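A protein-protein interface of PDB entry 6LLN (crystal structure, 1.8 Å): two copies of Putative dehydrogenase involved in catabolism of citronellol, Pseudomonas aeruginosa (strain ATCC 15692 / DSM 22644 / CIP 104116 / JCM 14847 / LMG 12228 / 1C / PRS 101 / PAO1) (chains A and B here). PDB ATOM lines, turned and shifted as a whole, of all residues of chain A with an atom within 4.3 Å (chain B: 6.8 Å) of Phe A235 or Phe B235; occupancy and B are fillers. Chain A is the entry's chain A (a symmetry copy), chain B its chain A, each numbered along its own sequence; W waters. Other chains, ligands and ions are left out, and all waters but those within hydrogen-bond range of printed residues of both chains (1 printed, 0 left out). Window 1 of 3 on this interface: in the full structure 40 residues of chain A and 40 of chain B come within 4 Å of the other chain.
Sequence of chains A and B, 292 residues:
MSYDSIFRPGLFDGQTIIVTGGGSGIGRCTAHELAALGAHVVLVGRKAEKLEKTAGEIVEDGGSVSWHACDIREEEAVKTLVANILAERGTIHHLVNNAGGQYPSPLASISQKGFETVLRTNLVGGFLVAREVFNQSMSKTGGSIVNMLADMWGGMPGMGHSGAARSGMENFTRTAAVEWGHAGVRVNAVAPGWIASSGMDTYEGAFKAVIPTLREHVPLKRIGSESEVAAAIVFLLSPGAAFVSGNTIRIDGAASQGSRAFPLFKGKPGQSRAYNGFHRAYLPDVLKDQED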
ATOM      1  N   ILE A   6      -9.706  11.586  23.378  1.00  0.00           N
ATOM      2  CA  ILE A   6     -10.606  12.726  23.213  1.00  0.00           C
ATOM      3  C   ILE A   6     -11.802  12.633  24.141  1.00  0.00           C
ATOM      4  O   ILE A   6     -12.550  13.607  24.273  1.00  0.00           O
ATOM      5  CB  ILE A   6     -11.069  12.845  21.746  1.00  0.00           C
ATOM      6  CG1 ILE A   6     -11.834  11.580  21.330  1.00  0.00           C
ATOM      7  CG2 ILE A   6      -9.874  13.100  20.822  1.00  0.00           C
ATOM      8  CD1 ILE A   6     -12.756  11.767  20.109  1.00  0.00           C
ATOM      9  N   PHE A   7     -12.006  11.486  24.788  1.00  0.00           N
ATOM     10  CA  PHE A   7     -13.185  11.228  25.601  1.00  0.00           C
ATOM     11  C   PHE A   7     -12.910  11.573  27.059  1.00  0.00           C
ATOM     12  O   PHE A   7     -11.765  11.563  27.509  1.00  0.00           O
ATOM     13  CB  PHE A   7     -13.624   9.762  25.458  1.00  0.00           C
ATOM     14  CG  PHE A   7     -13.962   9.390  24.035  1.00  0.00           C
ATOM     15  CD1 PHE A   7     -15.187   9.755  23.496  1.00  0.00           C
ATOM     16  CD2 PHE A   7     -13.044   8.724  23.228  1.00  0.00           C
ATOM     17  CE1 PHE A   7     -15.505   9.451  22.191  1.00  0.00           C
ATOM     18  CE2 PHE A   7     -13.365   8.409  21.902  1.00  0.00           C
ATOM     19  CZ  PHE A   7     -14.604   8.780  21.396  1.00  0.00           C
ATOM     20  N   ALA A 231     -10.321   5.543  18.130  1.00  0.00           N
ATOM     21  CA  ALA A 231     -11.243   6.575  18.586  1.00  0.00           C
ATOM     22  C   ALA A 231     -12.627   6.389  17.971  1.00  0.00           C
ATOM     23  O   ALA A 231     -13.642   6.648  18.630  1.00  0.00           O
ATOM     24  CB  ALA A 231     -10.685   7.971  18.281  1.00  0.00           C
ATOM     25  N   ALA A 232     -12.688   5.942  16.707  1.00  0.00           N
ATOM     26  CA  ALA A 232     -13.979   5.667  16.078  1.00  0.00           C
ATOM     27  C   ALA A 232     -14.673   4.480  16.736  1.00  0.00           C
ATOM     28  O   ALA A 232     -15.897   4.494  16.926  1.00  0.00           O
ATOM     29  CB  ALA A 232     -13.798   5.398  14.589  1.00  0.00           C
ATOM     30  N   ILE A 233     -13.915   3.433  17.060  1.00  0.00           N
ATOM     31  CA  ILE A 233     -14.498   2.290  17.754  1.00  0.00           C
ATOM     32  C   ILE A 233     -15.046   2.727  19.102  1.00  0.00           C
ATOM     33  O   ILE A 233     -16.176   2.383  19.478  1.00  0.00           O
ATOM     34  CB  ILE A 233     -13.463   1.165  17.921  1.00  0.00           C
ATOM     35  CG1 ILE A 233     -12.975   0.657  16.560  1.00  0.00           C
ATOM     36  CG2 ILE A 233     -14.054   0.027  18.781  1.00  0.00           C
ATOM     37  CD1 ILE A 233     -11.819  -0.379  16.705  1.00  0.00           C
ATOM     38  N   VAL A 234     -14.240   3.475  19.857  1.00  0.00           N
ATOM     39  CA  VAL A 234     -14.675   3.947  21.163  1.00  0.00           C
ATOM     40  C   VAL A 234     -15.903   4.838  21.030  1.00  0.00           C
ATOM     41  O   VAL A 234     -16.840   4.739  21.832  1.00  0.00           O
ATOM     42  CB  VAL A 234     -13.518   4.663  21.879  1.00  0.00           C
ATOM     43  CG1 VAL A 234     -13.996   5.295  23.197  1.00  0.00           C
ATOM     44  CG2 VAL A 234     -12.386   3.687  22.125  1.00  0.00           C
ATOM     45  N   PHE A 235     -15.935   5.710  20.013  1.00  0.00           N
ATOM     46  CA  PHE A 235     -17.132   6.528  19.841  1.00  0.00           C
ATOM     47  C   PHE A 235     -18.369   5.657  19.690  1.00  0.00           C
ATOM     48  O   PHE A 235     -19.425   5.953  20.260  1.00  0.00           O
ATOM     49  CB  PHE A 235     -17.049   7.442  18.616  1.00  0.00           C
ATOM     50  CG  PHE A 235     -18.356   8.124  18.331  1.00  0.00           C
ATOM     51  CD1 PHE A 235     -18.797   9.157  19.159  1.00  0.00           C
ATOM     52  CD2 PHE A 235     -19.177   7.698  17.290  1.00  0.00           C
ATOM     53  CE1 PHE A 235     -20.015   9.773  18.939  1.00  0.00           C
ATOM     54  CE2 PHE A 235     -20.395   8.322  17.057  1.00  0.00           C
ATOM     55  CZ  PHE A 235     -20.809   9.354  17.892  1.00  0.00           C
ATOM     56  N   LEU A 236     -18.266   4.597  18.898  1.00  0.00           N
ATOM     57  CA  LEU A 236     -19.436   3.768  18.623  1.00  0.00           C
ATOM     58  C   LEU A 236     -19.902   3.002  19.854  1.00  0.00           C
ATOM     59  O   LEU A 236     -21.070   2.606  19.907  1.00  0.00           O
ATOM     60  CB  LEU A 236     -19.136   2.781  17.496  1.00  0.00           C
ATOM     61  CG  LEU A 236     -19.052   3.446  16.122  1.00  0.00           C
ATOM     62  CD1 LEU A 236     -18.404   2.491  15.137  1.00  0.00           C
ATOM     63  CD2 LEU A 236     -20.417   3.918  15.625  1.00  0.00           C
ATOM     64  N   LEU A 237     -19.019   2.770  20.828  1.00  0.00           N
ATOM     65  CA  LEU A 237     -19.417   2.125  22.077  1.00  0.00           C
ATOM     66  C   LEU A 237     -20.000   3.109  23.086  1.00  0.00           C
ATOM     67  O   LEU A 237     -20.589   2.683  24.090  1.00  0.00           O
ATOM     68  CB  LEU A 237     -18.216   1.415  22.710  1.00  0.00           C
ATOM     69  CG  LEU A 237     -17.442   0.394  21.873  1.00  0.00           C
ATOM     70  CD1 LEU A 237     -16.228  -0.092  22.649  1.00  0.00           C
ATOM     71  CD2 LEU A 237     -18.335  -0.797  21.480  1.00  0.00           C
ATOM     72  N   SER A 238     -19.861   4.392  22.847  1.00  0.00           N
ATOM     73  CA  SER A 238     -20.137   5.395  23.857  1.00  0.00           C
ATOM     74  C   SER A 238     -21.606   5.784  23.871  1.00  0.00           C
ATOM     75  O   SER A 238     -22.350   5.495  22.930  1.00  0.00           O
ATOM     76  CB  SER A 238     -19.268   6.624  23.599  1.00  0.00           C
ATOM     77  OG  SER A 238     -19.808   7.384  22.535  1.00  0.00           O
ATOM     78  N   GLY A 240     -22.710   8.614  23.300  1.00  0.00           N
ATOM     79  CA  GLY A 240     -22.928   9.504  22.180  1.00  0.00           C
ATOM     80  C   GLY A 240     -23.434   8.801  20.940  1.00  0.00           C
ATOM     81  O   GLY A 240     -24.070   9.438  20.092  1.00  0.00           O
ATOM     82  N   ALA A 241     -23.173   7.499  20.816  1.00  0.00           N
ATOM     83  CA  ALA A 241     -23.633   6.701  19.691  1.00  0.00           C
ATOM     84  C   ALA A 241     -24.921   5.931  19.999  1.00  0.00           C
ATOM     85  O   ALA A 241     -25.235   4.953  19.309  1.00  0.00           O
ATOM     86  CB  ALA A 241     -22.528   5.735  19.252  1.00  0.00           C
ATOM     87  N   ILE B   6     -19.765  13.477  26.187  1.00  0.00           N
ATOM     88  CA  ILE B   6     -18.876  12.325  26.322  1.00  0.00           C
ATOM     89  C   ILE B   6     -17.425  12.711  26.112  1.00  0.00           C
ATOM     90  O   ILE B   6     -16.531  11.904  26.387  1.00  0.00           O
ATOM     91  CB  ILE B   6     -19.284  11.205  25.342  1.00  0.00           C
ATOM     92  CG1 ILE B   6     -19.183  11.709  23.894  1.00  0.00           C
ATOM     93  CG2 ILE B   6     -20.696  10.702  25.657  1.00  0.00           C
ATOM     94  CD1 ILE B   6     -19.072  10.591  22.838  1.00  0.00           C
ATOM     95  N   PHE B   7     -17.162  13.924  25.628  1.00  0.00           N
ATOM     96  CA  PHE B   7     -15.824  14.364  25.260  1.00  0.00           C
ATOM     97  C   PHE B   7     -15.166  15.091  26.425  1.00  0.00           C
ATOM     98  O   PHE B   7     -15.841  15.640  27.295  1.00  0.00           O
ATOM     99  CB  PHE B   7     -15.881  15.263  24.014  1.00  0.00           C
ATOM    100  CG  PHE B   7     -16.476  14.564  22.816  1.00  0.00           C
ATOM    101  CD1 PHE B   7     -15.705  13.677  22.078  1.00  0.00           C
ATOM    102  CD2 PHE B   7     -17.808  14.754  22.461  1.00  0.00           C
ATOM    103  CE1 PHE B   7     -16.237  13.006  20.999  1.00  0.00           C
ATOM    104  CE2 PHE B   7     -18.351  14.078  21.361  1.00  0.00           C
ATOM    105  CZ  PHE B   7     -17.550  13.204  20.637  1.00  0.00           C
ATOM    106  N   PHE B  12     -12.183  21.552  22.427  1.00  0.00           N
ATOM    107  CA  PHE B  12     -12.154  22.511  21.327  1.00  0.00           C
ATOM    108  C   PHE B  12     -11.725  23.906  21.782  1.00  0.00           C
ATOM    109  O   PHE B  12     -12.089  24.902  21.157  1.00  0.00           O
ATOM    110  CB  PHE B  12     -13.511  22.551  20.627  1.00  0.00           C
ATOM    111  CG  PHE B  12     -13.836  21.277  19.881  1.00  0.00           C
ATOM    112  CD1 PHE B  12     -13.374  21.079  18.592  1.00  0.00           C
ATOM    113  CD2 PHE B  12     -14.581  20.272  20.487  1.00  0.00           C
ATOM    114  CE1 PHE B  12     -13.650  19.889  17.907  1.00  0.00           C
ATOM    115  CE2 PHE B  12     -14.873  19.088  19.812  1.00  0.00           C
ATOM    116  CZ  PHE B  12     -14.407  18.894  18.525  1.00  0.00           C
ATOM    117  N   VAL B 146     -18.665  19.272   8.417  1.00  0.00           N
ATOM    118  CA  VAL B 146     -19.703  18.251   8.559  1.00  0.00           C
ATOM    119  C   VAL B 146     -20.987  18.790   7.938  1.00  0.00           C
ATOM    120  O   VAL B 146     -21.477  19.863   8.325  1.00  0.00           O
ATOM    121  CB  VAL B 146     -19.941  17.852  10.029  1.00  0.00           C
ATOM    122  CG1 VAL B 146     -21.146  16.905  10.117  1.00  0.00           C
ATOM    123  CG2 VAL B 146     -18.699  17.191  10.616  1.00  0.00           C
ATOM    124  N   ARG B 186     -10.902  17.794   5.988  1.00  0.00           N
ATOM    125  CA  ARG B 186     -11.770  16.625   6.012  1.00  0.00           C
ATOM    126  C   ARG B 186     -13.210  17.064   5.797  1.00  0.00           C
ATOM    127  O   ARG B 186     -13.633  18.103   6.302  1.00  0.00           O
ATOM    128  CB  ARG B 186     -11.643  15.884   7.344  1.00  0.00           C
ATOM    129  CG  ARG B 186     -10.231  15.426   7.660  1.00  0.00           C
ATOM    130  CD  ARG B 186     -10.176  14.647   8.977  1.00  0.00           C
ATOM    131  NE  ARG B 186     -10.536  15.475  10.124  1.00  0.00           N
ATOM    132  CZ  ARG B 186     -11.719  15.426  10.739  1.00  0.00           C
ATOM    133  NH1 ARG B 186     -12.662  14.583  10.318  1.00  0.00           N
ATOM    134  NH2 ARG B 186     -11.956  16.212  11.781  1.00  0.00           N
ATOM    135  N   GLU B 228     -28.079  12.941  20.473  1.00  0.00           N
ATOM    136  CA  GLU B 228     -27.584  11.752  19.793  1.00  0.00           C
ATOM    137  C   GLU B 228     -27.126  12.056  18.371  1.00  0.00           C
ATOM    138  O   GLU B 228     -26.359  11.273  17.803  1.00  0.00           O
ATOM    139  CB  GLU B 228     -28.668  10.669  19.832  1.00  0.00           C
ATOM    140  CG  GLU B 228     -28.767  10.021  21.225  1.00  0.00           C
ATOM    141  CD  GLU B 228     -29.991   9.139  21.434  1.00  0.00           C
ATOM    142  OE1 GLU B 228     -30.983   9.267  20.684  1.00  0.00           O
ATOM    143  OE2 GLU B 228     -29.960   8.317  22.384  1.00  0.00           O
ATOM    144  N   VAL B 229     -27.551  13.180  17.796  1.00  0.00           N
ATOM    145  CA  VAL B 229     -26.972  13.651  16.538  1.00  0.00           C
ATOM    146  C   VAL B 229     -25.743  14.514  16.797  1.00  0.00           C
ATOM    147  O   VAL B 229     -24.715  14.344  16.140  1.00  0.00           O
ATOM    148  CB  VAL B 229     -28.027  14.405  15.704  1.00  0.00           C
ATOM    149  CG1 VAL B 229     -27.425  14.860  14.364  1.00  0.00           C
ATOM    150  CG2 VAL B 229     -29.241  13.515  15.467  1.00  0.00           C
ATOM    151  N   ALA B 230     -25.815  15.411  17.788  1.00  0.00           N
ATOM    152  CA  ALA B 230     -24.712  16.333  18.052  1.00  0.00           C
ATOM    153  C   ALA B 230     -23.428  15.590  18.388  1.00  0.00           C
ATOM    154  O   ALA B 230     -22.343  15.977  17.934  1.00  0.00           O
ATOM    155  CB  ALA B 230     -25.080  17.290  19.188  1.00  0.00           C
ATOM    156  N   ALA B 231     -23.520  14.506  19.168  1.00  0.00           N
ATOM    157  CA  ALA B 231     -22.295  13.821  19.561  1.00  0.00           C
ATOM    158  C   ALA B 231     -21.563  13.260  18.346  1.00  0.00           C
ATOM    159  O   ALA B 231     -20.325  13.256  18.310  1.00  0.00           O
ATOM    160  CB  ALA B 231     -22.598  12.719  20.583  1.00  0.00           C
ATOM    161  N   ALA B 232     -22.310  12.779  17.340  1.00  0.00           N
ATOM    162  CA  ALA B 232     -21.680  12.295  16.112  1.00  0.00           C
ATOM    163  C   ALA B 232     -21.027  13.436  15.339  1.00  0.00           C
ATOM    164  O   ALA B 232     -19.936  13.270  14.778  1.00  0.00           O
ATOM    165  CB  ALA B 232     -22.706  11.595  15.229  1.00  0.00           C
ATOM    166  N   ILE B 233     -21.694  14.587  15.272  1.00  0.00           N
ATOM    167  CA  ILE B 233     -21.100  15.743  14.608  1.00  0.00           C
ATOM    168  C   ILE B 233     -19.819  16.146  15.318  1.00  0.00           C
ATOM    169  O   ILE B 233     -18.781  16.385  14.684  1.00  0.00           O
ATOM    170  CB  ILE B 233     -22.093  16.915  14.559  1.00  0.00           C
ATOM    171  CG1 ILE B 233     -23.349  16.543  13.763  1.00  0.00           C
ATOM    172  CG2 ILE B 233     -21.401  18.170  13.983  1.00  0.00           C
ATOM    173  CD1 ILE B 233     -24.432  17.663  13.825  1.00  0.00           C
ATOM    174  N   VAL B 234     -19.883  16.250  16.646  1.00  0.00           N
ATOM    175  CA  VAL B 234     -18.708  16.627  17.418  1.00  0.00           C
ATOM    176  C   VAL B 234     -17.594  15.606  17.232  1.00  0.00           C
ATOM    177  O   VAL B 234     -16.421  15.975  17.092  1.00  0.00           O
ATOM    178  CB  VAL B 234     -19.084  16.808  18.898  1.00  0.00           C
ATOM    179  CG1 VAL B 234     -17.831  17.064  19.754  1.00  0.00           C
ATOM    180  CG2 VAL B 234     -20.078  17.943  19.039  1.00  0.00           C
ATOM    181  N   PHE B 235     -17.932  14.309  17.211  1.00  0.00           N
ATOM    182  CA  PHE B 235     -16.880  13.324  16.974  1.00  0.00           C
ATOM    183  C   PHE B 235     -16.165  13.597  15.660  1.00  0.00           C
ATOM    184  O   PHE B 235     -14.935  13.499  15.577  1.00  0.00           O
ATOM    185  CB  PHE B 235     -17.416  11.891  16.929  1.00  0.00           C
ATOM    186  CG  PHE B 235     -16.368  10.911  16.484  1.00  0.00           C
ATOM    187  CD1 PHE B 235     -15.326  10.568  17.346  1.00  0.00           C
ATOM    188  CD2 PHE B 235     -16.378  10.385  15.195  1.00  0.00           C
ATOM    189  CE1 PHE B 235     -14.329   9.698  16.945  1.00  0.00           C
ATOM    190  CE2 PHE B 235     -15.386   9.501  14.792  1.00  0.00           C
ATOM    191  CZ  PHE B 235     -14.361   9.169  15.671  1.00  0.00           C
ATOM    192  N   LEU B 236     -16.922  13.906  14.615  1.00  0.00           N
ATOM    193  CA  LEU B 236     -16.319  14.084  13.298  1.00  0.00           C
ATOM    194  C   LEU B 236     -15.439  15.325  13.229  1.00  0.00           C
ATOM    195  O   LEU B 236     -14.560  15.390  12.365  1.00  0.00           O
ATOM    196  CB  LEU B 236     -17.403  14.172  12.224  1.00  0.00           C
ATOM    197  CG  LEU B 236     -18.077  12.830  11.940  1.00  0.00           C
ATOM    198  CD1 LEU B 236     -19.356  13.062  11.156  1.00  0.00           C
ATOM    199  CD2 LEU B 236     -17.148  11.859  11.216  1.00  0.00           C
ATOM    200  N   LEU B 237     -15.666  16.311  14.100  1.00  0.00           N
ATOM    201  CA  LEU B 237     -14.803  17.489  14.155  1.00  0.00           C
ATOM    202  C   LEU B 237     -13.557  17.265  15.006  1.00  0.00           C
ATOM    203  O   LEU B 237     -12.627  18.083  14.961  1.00  0.00           O
ATOM    204  CB  LEU B 237     -15.580  18.686  14.713  1.00  0.00           C
ATOM    205  CG  LEU B 237     -16.892  19.088  14.038  1.00  0.00           C
ATOM    206  CD1 LEU B 237     -17.550  20.213  14.823  1.00  0.00           C
ATOM    207  CD2 LEU B 237     -16.658  19.523  12.579  1.00  0.00           C
ATOM    208  N   SER B 238     -13.512  16.194  15.763  1.00  0.00           N
ATOM    209  CA  SER B 238     -12.509  16.026  16.796  1.00  0.00           C
ATOM    210  C   SER B 238     -11.232  15.415  16.240  1.00  0.00           C
ATOM    211  O   SER B 238     -11.217  14.868  15.135  1.00  0.00           O
ATOM    212  CB  SER B 238     -13.073  15.146  17.910  1.00  0.00           C
ATOM    213  OG  SER B 238     -13.053  13.789  17.512  1.00  0.00           O
ATOM    214  N   PRO B 239     -10.131  15.486  17.000  1.00  0.00           N
ATOM    215  CA  PRO B 239      -8.899  14.810  16.569  1.00  0.00           C
ATOM    216  C   PRO B 239      -9.061  13.313  16.414  1.00  0.00           C
ATOM    217  O   PRO B 239      -8.298  12.694  15.664  1.00  0.00           O
ATOM    218  CB  PRO B 239      -7.902  15.145  17.687  1.00  0.00           C
ATOM    219  CG  PRO B 239      -8.418  16.396  18.295  1.00  0.00           C
ATOM    220  CD  PRO B 239      -9.915  16.307  18.207  1.00  0.00           C
ATOM    221  N   GLY B 240     -10.022  12.707  17.109  1.00  0.00           N
ATOM    222  CA  GLY B 240     -10.263  11.289  16.940  1.00  0.00           C
ATOM    223  C   GLY B 240     -10.697  10.914  15.540  1.00  0.00           C
ATOM    224  O   GLY B 240     -10.510   9.763  15.130  1.00  0.00           O
ATOM    225  N   ALA B 241     -11.269  11.861  14.794  1.00  0.00           N
ATOM    226  CA  ALA B 241     -11.698  11.638  13.422  1.00  0.00           C
ATOM    227  C   ALA B 241     -10.666  12.114  12.395  1.00  0.00           C
ATOM    228  O   ALA B 241     -11.013  12.333  11.228  1.00  0.00           O
ATOM    229  CB  ALA B 241     -13.045  12.327  13.182  1.00  0.00           C
ATOM    230  N   ALA B 242      -9.392  12.231  12.792  1.00  0.00           N
ATOM    231  CA  ALA B 242      -8.393  12.862  11.924  1.00  0.00           C
ATOM    232  C   ALA B 242      -8.145  12.106  10.620  1.00  0.00           C
ATOM    233  O   ALA B 242      -7.631  12.703   9.669  1.00  0.00           O
ATOM    234  CB  ALA B 242      -7.068  13.024  12.679  1.00  0.00           C
ATOM    235  N   VAL B 244     -10.758  10.294   9.205  1.00  0.00           N
ATOM    236  CA  VAL B 244     -12.111  10.076   8.699  1.00  0.00           C
ATOM    237  C   VAL B 244     -12.457  11.224   7.763  1.00  0.00           C
ATOM    238  O   VAL B 244     -12.547  12.376   8.202  1.00  0.00           O
ATOM    239  CB  VAL B 244     -13.141   9.996   9.840  1.00  0.00           C
ATOM    240  CG1 VAL B 244     -14.545   9.789   9.242  1.00  0.00           C
ATOM    241  CG2 VAL B 244     -12.792   8.881  10.810  1.00  0.00           C
ATOM    242  N   ILE B 249     -22.048   9.369   8.848  1.00  0.00           N
ATOM    243  CA  ILE B 249     -22.579   8.606   9.980  1.00  0.00           C
ATOM    244  C   ILE B 249     -24.104   8.675   9.928  1.00  0.00           C
ATOM    245  O   ILE B 249     -24.691   9.759  10.005  1.00  0.00           O
ATOM    246  CB  ILE B 249     -22.036   9.125  11.322  1.00  0.00           C
ATOM    247  CG1 ILE B 249     -20.508   8.967  11.391  1.00  0.00           C
ATOM    248  CG2 ILE B 249     -22.697   8.375  12.516  1.00  0.00           C
ATOM    249  CD1 ILE B 249     -19.855   9.491  12.698  1.00  0.00           C
ATOM    250  N   ILE B 251     -27.515   8.193  11.825  1.00  0.00           N
ATOM    251  CA  ILE B 251     -28.019   8.190  13.196  1.00  0.00           C
ATOM    252  C   ILE B 251     -29.521   7.943  13.124  1.00  0.00           C
ATOM    253  O   ILE B 251     -30.324   8.884  13.182  1.00  0.00           O
ATOM    254  CB  ILE B 251     -27.692   9.507  13.923  1.00  0.00           C
ATOM    255  CG1 ILE B 251     -26.184   9.775  13.868  1.00  0.00           C
ATOM    256  CG2 ILE B 251     -28.139   9.431  15.390  1.00  0.00           C
ATOM    257  CD1 ILE B 251     -25.801  11.132  13.315  1.00  0.00           C
HETATM  258  O   HOH W   1     -26.155   8.624  18.672  1.00  0.00           O
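O of Phe B235 lies within hydrogen-bond range of OG of Ser B238, at 2.7 Å. The side-chain hydroxyl (OG) of Ser B238 lies close to the backbone NH (N) of Gly B240 (3.2 Å). The backbone carbonyl oxygen of Phe A235 is in hydrogen-bond range of the side-chain hydroxyl of Ser A238 (2.7 Å). The backbone NH (N) of Gly A240 sits close to the side-chain hydroxyl (OG) of Ser A238 (3.2 Å).
Among the printed residues, pairs that only touch across the chains: Ser A238 with Ile B6, Ile A6 with Ser B238, Ile A6 with Phe B7, Phe A7 with Ile B6, Ala A232 with Phe B235, Phe A235 with Ala B232, Ala A231 with Phe B235, Phe A235 with Ala B231, Ala A231 with Gly B240, Gly A240 with Ala B231, Gly A240 with Glu B228, Ile A6 with Gly B240, Gly A240 with Ile B6, Phe A235 with Phe B235, Phe A7 with Phe B7, Phe A235 with Ile B6 and Ile A6 with Phe B235.
Printed residues of chain B within 4 Å of Phe A7: Ile B6 and Phe B7. Of the printed residues of chain B, Gly A240 touches Ile B6, Glu B228 and Ala B231. Printed residues of chain A within 4 Å of Glu B228: Gly A240 (3.7 Å). Of the printed residues of chain A, Ala B232 touches Phe A235. Of the printed residues of chain A, Ser B238 touches Ile A6 (3.3 Å). Ala B241 touches none of the printed residues of chain A.
Of the 23 printed residues of chain B, 8 touch a printed residue of chain A. Along chain B the printed residues that touch a printed residue of chain A span positions 6 to 240. Along chain A the printed residues that touch a printed residue of chain B span positions 6 to 240. Among the printed residues, no Asp or Glu carboxylate lies within 4 Å of a Lys or Arg side-chain nitrogen of the other chain.
Ile A6 touches Phe B7, and with the chains exchanged Phe A7 touches Ile B6. Phe A7 touches its own counterpart, Phe B7. Ala A231 touches Phe B235, and with the chains exchanged Phe A235 touches Ala B231. Phe B235 touches its own counterpart, Phe A235. 12 positions are printed for both chains. Of the 17 pairs that touch across the chains among the printed residues, 16 have their exchanged pair printed and touching as well.
Water W1 bridges O of Gly A240 and O of Glu B228.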
